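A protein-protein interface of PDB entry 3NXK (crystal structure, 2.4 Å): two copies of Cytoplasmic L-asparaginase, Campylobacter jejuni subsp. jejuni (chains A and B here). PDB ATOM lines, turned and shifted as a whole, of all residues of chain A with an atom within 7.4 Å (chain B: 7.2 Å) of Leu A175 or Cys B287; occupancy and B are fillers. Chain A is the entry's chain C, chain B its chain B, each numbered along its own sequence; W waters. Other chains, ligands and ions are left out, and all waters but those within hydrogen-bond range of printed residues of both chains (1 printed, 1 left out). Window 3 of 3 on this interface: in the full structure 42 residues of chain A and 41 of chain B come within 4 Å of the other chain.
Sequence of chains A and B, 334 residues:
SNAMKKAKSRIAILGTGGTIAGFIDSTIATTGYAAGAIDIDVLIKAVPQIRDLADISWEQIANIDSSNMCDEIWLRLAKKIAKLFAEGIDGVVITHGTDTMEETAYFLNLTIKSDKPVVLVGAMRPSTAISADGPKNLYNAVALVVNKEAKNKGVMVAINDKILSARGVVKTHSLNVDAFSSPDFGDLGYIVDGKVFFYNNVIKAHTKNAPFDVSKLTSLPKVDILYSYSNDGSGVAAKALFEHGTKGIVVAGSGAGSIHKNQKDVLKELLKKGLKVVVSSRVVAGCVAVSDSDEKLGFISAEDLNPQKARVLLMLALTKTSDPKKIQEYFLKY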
ATOM      1  N   THR A  30     -10.167   6.160 -27.558  1.00  0.00           N
ATOM      2  CA  THR A  30      -9.101   5.619 -26.723  1.00  0.00           C
ATOM      3  C   THR A  30      -7.716   5.778 -27.359  1.00  0.00           C
ATOM      4  O   THR A  30      -6.708   5.738 -26.655  1.00  0.00           O
ATOM      5  CB  THR A  30      -9.346   4.120 -26.397  1.00  0.00           C
ATOM      6  OG1 THR A  30     -10.038   4.004 -25.146  1.00  0.00           O
ATOM      7  CG2 THR A  30      -8.030   3.348 -26.318  1.00  0.00           C
ATOM      8  N   THR A  31      -7.651   5.953 -28.679  1.00  0.00           N
ATOM      9  CA  THR A  31      -6.344   6.019 -29.345  1.00  0.00           C
ATOM     10  C   THR A  31      -5.749   7.426 -29.408  1.00  0.00           C
ATOM     11  O   THR A  31      -4.573   7.616 -29.083  1.00  0.00           O
ATOM     12  CB  THR A  31      -6.338   5.375 -30.768  1.00  0.00           C
ATOM     13  OG1 THR A  31      -7.551   5.692 -31.464  1.00  0.00           O
ATOM     14  CG2 THR A  31      -6.183   3.856 -30.684  1.00  0.00           C
ATOM     15  N   MET A 124      -4.920   2.284 -19.312  1.00  0.00           N
ATOM     16  CA  MET A 124      -4.782   2.071 -20.742  1.00  0.00           C
ATOM     17  C   MET A 124      -5.751   2.948 -21.501  1.00  0.00           C
ATOM     18  O   MET A 124      -5.581   3.183 -22.687  1.00  0.00           O
ATOM     19  CB  MET A 124      -4.970   0.598 -21.105  1.00  0.00           C
ATOM     20  CG  MET A 124      -3.789  -0.269 -20.686  1.00  0.00           C
ATOM     21  SD  MET A 124      -2.083   0.274 -21.510  1.00  0.00           S
ATOM     22  CE  MET A 124      -2.388  -0.382 -23.333  1.00  0.00           C
ATOM     23  N   ARG A 125      -6.763   3.436 -20.793  1.00  0.00           N
ATOM     24  CA  ARG A 125      -7.787   4.296 -21.370  1.00  0.00           C
ATOM     25  C   ARG A 125      -7.737   5.660 -20.706  1.00  0.00           C
ATOM     26  O   ARG A 125      -7.460   5.765 -19.502  1.00  0.00           O
ATOM     27  CB  ARG A 125      -9.178   3.678 -21.186  1.00  0.00           C
ATOM     28  CG  ARG A 125      -9.370   2.416 -21.993  1.00  0.00           C
ATOM     29  CD  ARG A 125     -10.757   1.822 -21.814  1.00  0.00           C
ATOM     30  NE  ARG A 125     -10.852   0.501 -22.434  1.00  0.00           N
ATOM     31  CZ  ARG A 125     -11.647  -0.466 -21.987  1.00  0.00           C
ATOM     32  NH1 ARG A 125     -12.407  -0.254 -20.915  1.00  0.00           N
ATOM     33  NH2 ARG A 125     -11.679  -1.645 -22.605  1.00  0.00           N
ATOM     34  N   LYS A 171       5.391  -4.290 -20.300  1.00  0.00           N
ATOM     35  CA  LYS A 171       4.165  -4.104 -21.045  1.00  0.00           C
ATOM     36  C   LYS A 171       4.170  -5.164 -22.123  1.00  0.00           C
ATOM     37  O   LYS A 171       5.157  -5.311 -22.843  1.00  0.00           O
ATOM     38  CB  LYS A 171       4.133  -2.725 -21.671  1.00  0.00           C
ATOM     39  CG  LYS A 171       2.780  -2.332 -22.233  1.00  0.00           C
ATOM     40  CD  LYS A 171       2.767  -0.853 -22.555  1.00  0.00           C
ATOM     41  CE  LYS A 171       1.374  -0.360 -22.891  1.00  0.00           C
ATOM     42  NZ  LYS A 171       1.405   1.124 -23.040  1.00  0.00           N
ATOM     43  N   THR A 172       3.089  -5.929 -22.213  1.00  0.00           N
ATOM     44  CA  THR A 172       3.038  -7.033 -23.169  1.00  0.00           C
ATOM     45  C   THR A 172       1.797  -6.944 -24.046  1.00  0.00           C
ATOM     46  O   THR A 172       1.521  -7.826 -24.873  1.00  0.00           O
ATOM     47  CB  THR A 172       3.142  -8.413 -22.473  1.00  0.00           C
ATOM     48  OG1 THR A 172       2.184  -8.502 -21.412  1.00  0.00           O
ATOM     49  CG2 THR A 172       4.542  -8.619 -21.900  1.00  0.00           C
ATOM     50  N   HIS A 173       1.040  -5.870 -23.855  1.00  0.00           N
ATOM     51  CA  HIS A 173      -0.029  -5.547 -24.784  1.00  0.00           C
ATOM     52  C   HIS A 173      -0.176  -4.043 -24.935  1.00  0.00           C
ATOM     53  O   HIS A 173      -0.169  -3.311 -23.953  1.00  0.00           O
ATOM     54  CB  HIS A 173      -1.358  -6.199 -24.398  1.00  0.00           C
ATOM     55  CG  HIS A 173      -2.318  -6.279 -25.540  1.00  0.00           C
ATOM     56  ND1 HIS A 173      -2.948  -5.167 -26.057  1.00  0.00           N
ATOM     57  CD2 HIS A 173      -2.715  -7.327 -26.305  1.00  0.00           C
ATOM     58  CE1 HIS A 173      -3.711  -5.528 -27.073  1.00  0.00           C
ATOM     59  NE2 HIS A 173      -3.586  -6.832 -27.246  1.00  0.00           N
ATOM     60  N   SER A 174      -0.322  -3.587 -26.176  1.00  0.00           N
ATOM     61  CA  SER A 174      -0.283  -2.156 -26.473  1.00  0.00           C
ATOM     62  C   SER A 174      -1.646  -1.465 -26.398  1.00  0.00           C
ATOM     63  O   SER A 174      -1.707  -0.250 -26.371  1.00  0.00           O
ATOM     64  CB  SER A 174       0.394  -1.887 -27.833  1.00  0.00           C
ATOM     65  OG  SER A 174      -0.243  -2.572 -28.908  1.00  0.00           O
ATOM     66  N   LEU A 175      -2.725  -2.237 -26.346  1.00  0.00           N
ATOM     67  CA  LEU A 175      -4.068  -1.667 -26.393  1.00  0.00           C
ATOM     68  C   LEU A 175      -4.992  -2.154 -25.295  1.00  0.00           C
ATOM     69  O   LEU A 175      -5.940  -1.454 -24.933  1.00  0.00           O
ATOM     70  CB  LEU A 175      -4.741  -1.933 -27.749  1.00  0.00           C
ATOM     71  CG  LEU A 175      -4.210  -1.114 -28.929  1.00  0.00           C
ATOM     72  CD1 LEU A 175      -4.918  -1.494 -30.232  1.00  0.00           C
ATOM     73  CD2 LEU A 175      -4.321   0.390 -28.653  1.00  0.00           C
ATOM     74  N   ASN A 176      -4.750  -3.352 -24.773  1.00  0.00           N
ATOM     75  CA  ASN A 176      -5.729  -3.954 -23.871  1.00  0.00           C
ATOM     76  C   ASN A 176      -5.525  -3.489 -22.423  1.00  0.00           C
ATOM     77  O   ASN A 176      -4.403  -3.272 -21.995  1.00  0.00           O
ATOM     78  CB  ASN A 176      -5.676  -5.471 -24.001  1.00  0.00           C
ATOM     79  CG  ASN A 176      -6.904  -6.149 -23.451  1.00  0.00           C
ATOM     80  OD1 ASN A 176      -7.031  -6.326 -22.238  1.00  0.00           O
ATOM     81  ND2 ASN A 176      -7.814  -6.554 -24.346  1.00  0.00           N
ATOM     82  N   VAL A 177      -6.604  -3.316 -21.670  1.00  0.00           N
ATOM     83  CA  VAL A 177      -6.455  -2.927 -20.273  1.00  0.00           C
ATOM     84  C   VAL A 177      -5.625  -3.968 -19.504  1.00  0.00           C
ATOM     85  O   VAL A 177      -5.015  -3.665 -18.479  1.00  0.00           O
ATOM     86  CB  VAL A 177      -7.812  -2.690 -19.593  1.00  0.00           C
ATOM     87  CG1 VAL A 177      -8.620  -1.658 -20.383  1.00  0.00           C
ATOM     88  CG2 VAL A 177      -8.576  -4.003 -19.479  1.00  0.00           C
ATOM     89  N   ASP A 178      -5.585  -5.193 -20.012  1.00  0.00           N
ATOM     90  CA  ASP A 178      -4.716  -6.210 -19.432  1.00  0.00           C
ATOM     91  C   ASP A 178      -3.364  -6.110 -20.144  1.00  0.00           C
ATOM     92  O   ASP A 178      -3.048  -6.881 -21.040  1.00  0.00           O
ATOM     93  CB  ASP A 178      -5.348  -7.598 -19.588  1.00  0.00           C
ATOM     94  CG  ASP A 178      -4.607  -8.684 -18.819  1.00  0.00           C
ATOM     95  OD1 ASP A 178      -3.968  -8.369 -17.788  1.00  0.00           O
ATOM     96  OD2 ASP A 178      -4.685  -9.858 -19.252  1.00  0.00           O
ATOM     97  N   ALA A 179      -2.569  -5.141 -19.730  1.00  0.00           N
ATOM     98  CA  ALA A 179      -1.476  -4.668 -20.546  1.00  0.00           C
ATOM     99  C   ALA A 179      -0.109  -5.113 -20.023  1.00  0.00           C
ATOM    100  O   ALA A 179       0.893  -5.069 -20.757  1.00  0.00           O
ATOM    101  CB  ALA A 179      -1.556  -3.116 -20.635  1.00  0.00           C
ATOM    102  N   ASP B 184      -1.080 -12.313 -31.570  1.00  0.00           N
ATOM    103  CA  ASP B 184      -2.316 -11.669 -31.976  1.00  0.00           C
ATOM    104  C   ASP B 184      -3.283 -12.572 -32.741  1.00  0.00           C
ATOM    105  O   ASP B 184      -4.498 -12.447 -32.598  1.00  0.00           O
ATOM    106  CB  ASP B 184      -1.995 -10.398 -32.769  1.00  0.00           C
ATOM    107  CG  ASP B 184      -1.068  -9.451 -32.002  1.00  0.00           C
ATOM    108  OD1 ASP B 184      -1.533  -8.874 -30.995  1.00  0.00           O
ATOM    109  OD2 ASP B 184       0.118  -9.273 -32.394  1.00  0.00           O
ATOM    110  N   GLY B 255       4.867   1.223 -26.111  1.00  0.00           N
ATOM    111  CA  GLY B 255       3.434   1.005 -26.168  1.00  0.00           C
ATOM    112  C   GLY B 255       2.925   0.947 -27.595  1.00  0.00           C
ATOM    113  O   GLY B 255       3.430   0.181 -28.414  1.00  0.00           O
ATOM    114  N   ALA B 256       1.922   1.751 -27.910  1.00  0.00           N
ATOM    115  CA  ALA B 256       1.248   1.585 -29.195  1.00  0.00           C
ATOM    116  C   ALA B 256       1.907   2.394 -30.309  1.00  0.00           C
ATOM    117  O   ALA B 256       1.233   3.052 -31.092  1.00  0.00           O
ATOM    118  CB  ALA B 256      -0.261   1.886 -29.077  1.00  0.00           C
ATOM    119  N   GLY B 257       3.232   2.327 -30.373  1.00  0.00           N
ATOM    120  CA  GLY B 257       3.987   2.982 -31.426  1.00  0.00           C
ATOM    121  C   GLY B 257       4.405   4.399 -31.062  1.00  0.00           C
ATOM    122  O   GLY B 257       4.655   5.231 -31.925  1.00  0.00           O
ATOM    123  N   SER B 281       6.306  -1.588 -32.669  1.00  0.00           N
ATOM    124  CA  SER B 281       6.267  -1.568 -31.206  1.00  0.00           C
ATOM    125  C   SER B 281       7.216  -2.589 -30.584  1.00  0.00           C
ATOM    126  O   SER B 281       7.357  -3.706 -31.096  1.00  0.00           O
ATOM    127  CB  SER B 281       4.823  -1.824 -30.723  1.00  0.00           C
ATOM    128  OG  SER B 281       4.720  -1.946 -29.306  1.00  0.00           O
ATOM    129  N   VAL B 283       6.456  -3.845 -27.918  1.00  0.00           N
ATOM    130  CA  VAL B 283       5.477  -4.613 -27.169  1.00  0.00           C
ATOM    131  C   VAL B 283       4.985  -5.808 -27.989  1.00  0.00           C
ATOM    132  O   VAL B 283       4.575  -5.648 -29.130  1.00  0.00           O
ATOM    133  CB  VAL B 283       4.296  -3.709 -26.786  1.00  0.00           C
ATOM    134  CG1 VAL B 283       3.250  -4.484 -26.002  1.00  0.00           C
ATOM    135  CG2 VAL B 283       4.811  -2.505 -26.011  1.00  0.00           C
ATOM    136  N   ALA B 285       2.359  -8.067 -28.053  1.00  0.00           N
ATOM    137  CA  ALA B 285       1.004  -8.170 -28.612  1.00  0.00           C
ATOM    138  C   ALA B 285       0.322  -6.807 -28.709  1.00  0.00           C
ATOM    139  O   ALA B 285       0.768  -5.843 -28.088  1.00  0.00           O
ATOM    140  CB  ALA B 285       0.166  -9.122 -27.801  1.00  0.00           C
ATOM    141  N   GLY B 286      -0.762  -6.733 -29.478  1.00  0.00           N
ATOM    142  CA  GLY B 286      -1.434  -5.471 -29.730  1.00  0.00           C
ATOM    143  C   GLY B 286      -1.141  -4.834 -31.093  1.00  0.00           C
ATOM    144  O   GLY B 286      -0.385  -5.359 -31.906  1.00  0.00           O
ATOM    145  N   CYS B 287      -1.726  -3.667 -31.322  1.00  0.00           N
ATOM    146  CA  CYS B 287      -1.700  -3.014 -32.618  1.00  0.00           C
ATOM    147  C   CYS B 287      -1.261  -1.560 -32.416  1.00  0.00           C
ATOM    148  O   CYS B 287      -1.572  -0.952 -31.407  1.00  0.00           O
ATOM    149  CB  CYS B 287      -3.108  -3.114 -33.237  1.00  0.00           C
ATOM    150  SG  CYS B 287      -3.287  -2.673 -34.949  1.00  0.00           S
ATOM    151  N   VAL B 288      -0.510  -1.026 -33.369  1.00  0.00           N
ATOM    152  CA  VAL B 288       0.059   0.324 -33.287  1.00  0.00           C
ATOM    153  C   VAL B 288      -0.943   1.416 -33.673  1.00  0.00           C
ATOM    154  O   VAL B 288      -1.828   1.188 -34.498  1.00  0.00           O
ATOM    155  CB  VAL B 288       1.281   0.431 -34.224  1.00  0.00           C
ATOM    156  CG1 VAL B 288       1.407   1.816 -34.773  1.00  0.00           C
ATOM    157  CG2 VAL B 288       2.550   0.005 -33.494  1.00  0.00           C
ATOM    158  N   ALA B 289      -0.795   2.606 -33.089  1.00  0.00           N
ATOM    159  CA  ALA B 289      -1.674   3.736 -33.398  1.00  0.00           C
ATOM    160  C   ALA B 289      -0.910   4.934 -33.980  1.00  0.00           C
ATOM    161  O   ALA B 289       0.020   5.435 -33.354  1.00  0.00           O
ATOM    162  CB  ALA B 289      -2.431   4.168 -32.138  1.00  0.00           C
ATOM    163  N   SER B 301       1.835   3.256 -40.021  1.00  0.00           N
ATOM    164  CA  SER B 301       1.559   2.290 -38.947  1.00  0.00           C
ATOM    165  C   SER B 301       1.891   0.860 -39.368  1.00  0.00           C
ATOM    166  O   SER B 301       1.452   0.409 -40.424  1.00  0.00           O
ATOM    167  CB  SER B 301       0.082   2.330 -38.569  1.00  0.00           C
ATOM    168  OG  SER B 301      -0.277   1.161 -37.835  1.00  0.00           O
ATOM    169  N   ALA B 302       2.646   0.142 -38.548  1.00  0.00           N
ATOM    170  CA  ALA B 302       2.916  -1.270 -38.809  1.00  0.00           C
ATOM    171  C   ALA B 302       1.756  -2.147 -38.381  1.00  0.00           C
ATOM    172  O   ALA B 302       1.870  -3.374 -38.420  1.00  0.00           O
ATOM    173  CB  ALA B 302       4.135  -1.713 -38.061  1.00  0.00           C
ATOM    174  N   GLU B 303       0.665  -1.519 -37.944  1.00  0.00           N
ATOM    175  CA  GLU B 303      -0.437  -2.238 -37.304  1.00  0.00           C
ATOM    176  C   GLU B 303       0.086  -3.164 -36.205  1.00  0.00           C
ATOM    177  O   GLU B 303       0.705  -2.718 -35.221  1.00  0.00           O
ATOM    178  CB  GLU B 303      -1.216  -3.031 -38.346  1.00  0.00           C
ATOM    179  CG  GLU B 303      -1.552  -2.231 -39.585  1.00  0.00           C
ATOM    180  CD  GLU B 303      -2.425  -1.039 -39.276  1.00  0.00           C
ATOM    181  OE1 GLU B 303      -3.500  -1.237 -38.667  1.00  0.00           O
ATOM    182  OE2 GLU B 303      -2.040   0.092 -39.635  1.00  0.00           O
ATOM    183  N   ASP B 304      -0.125  -4.461 -36.380  1.00  0.00           N
ATOM    184  CA  ASP B 304       0.295  -5.426 -35.374  1.00  0.00           C
ATOM    185  C   ASP B 304       1.620  -6.112 -35.743  1.00  0.00           C
ATOM    186  O   ASP B 304       2.103  -6.989 -35.027  1.00  0.00           O
ATOM    187  CB  ASP B 304      -0.805  -6.456 -35.156  1.00  0.00           C
ATOM    188  CG  ASP B 304      -0.974  -7.358 -36.346  1.00  0.00           C
ATOM    189  OD1 ASP B 304      -1.479  -6.862 -37.386  1.00  0.00           O
ATOM    190  OD2 ASP B 304      -0.583  -8.548 -36.251  1.00  0.00           O
ATOM    191  N   LEU B 305       2.216  -5.703 -36.853  1.00  0.00           N
ATOM    192  CA  LEU B 305       3.490  -6.291 -37.261  1.00  0.00           C
ATOM    193  C   LEU B 305       4.652  -5.842 -36.385  1.00  0.00           C
ATOM    194  O   LEU B 305       4.893  -4.646 -36.244  1.00  0.00           O
ATOM    195  CB  LEU B 305       3.786  -5.966 -38.724  1.00  0.00           C
ATOM    196  CG  LEU B 305       3.042  -6.801 -39.769  1.00  0.00           C
ATOM    197  CD1 LEU B 305       3.447  -6.408 -41.176  1.00  0.00           C
ATOM    198  CD2 LEU B 305       3.308  -8.271 -39.552  1.00  0.00           C
HETATM  199  O   HOH W   1      -3.942  -8.940 -29.171  1.00  0.00           O
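The backbone NH of Cys B287 is in hydrogen-bond range of the side-chain hydroxyl of Ser A174.
The backbone NH (N) of Ala B285 lies within hydrogen-bond range of the backbone carbonyl oxygen (O) of Thr A172, 3.3 Å away.
The backbone NH (N) of Ser A174 lies within hydrogen-bond range of the backbone carbonyl oxygen (O) of Ala B285 (3.2 Å).
The backbone carbonyl oxygen (O) of Ala A179 sits at hydrogen-bond distance from the backbone NH (N) of Thr A172, at 2.8 Å.
The side-chain hydroxyl of Ser B281 sits at hydrogen-bond distance from the backbone carbonyl oxygen of Gly B255.
OG of Ser B281 is in hydrogen-bond range of N of Val B283 (2.9 Å).
A ring nitrogen (ND1) of His A173 sits at hydrogen-bond distance from the backbone NH of Leu A175 (3.0 Å).
The backbone NH (N) of Ala B289 lies within hydrogen-bond range of the backbone carbonyl oxygen (O) of Ala B256 (2.9 Å).
OD1 of Asp B184 is in hydrogen-bond range of N of Gly B286 (2.7 Å).
Among the printed residues, merely in contact across the chains: Ser A174 with Gly B286 (3.2 Å), His A173 with Val B283 (3.4 Å), His A173 with Ala B285 (3.4 Å), Thr A172 with Val B283 (3.5 Å), His A173 with Gly B286 (3.5 Å), Leu A175 with Cys B287 (3.6 Å), Ser A174 with Val B283 (3.7 Å), Ser A174 with Gly B255 (3.7 Å), Lys A171 with Gly B255 (3.7 Å), Ser A174 with Ala B256 (3.7 Å) and Lys A171 with Val B283 (3.8 Å).
Leu A175 touches just one residue of chain B: Cys B287.
Cys B287 touches two residues of chain A.
Of the printed residues of chain B, His A173 touches Val B283 (3.4 Å), Ala B285 (3.4 Å) and Gly B286 (3.5 Å).
Of the printed residues of chain B, Lys A171 touches Gly B255 (3.7 Å) and Val B283 (3.8 Å).
Ala A179 touches none of the printed residues of chain B.
Hydrophobic or aromatic side chains of chain A that line the printed part of chain B: His A173 and Leu A175.
Of the 16 printed residues of chain B, 6 touch a printed residue of chain A.
No position is printed for both chains.
Of the 14 pairs that touch across the chains among the printed residues, none has its exchanged pair printed and touching as well.
Water W1 bridges a ring nitrogen (NE2) of His A173 (2.9 Å) and the side-chain carboxylate of Asp B184 (3.0 Å).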
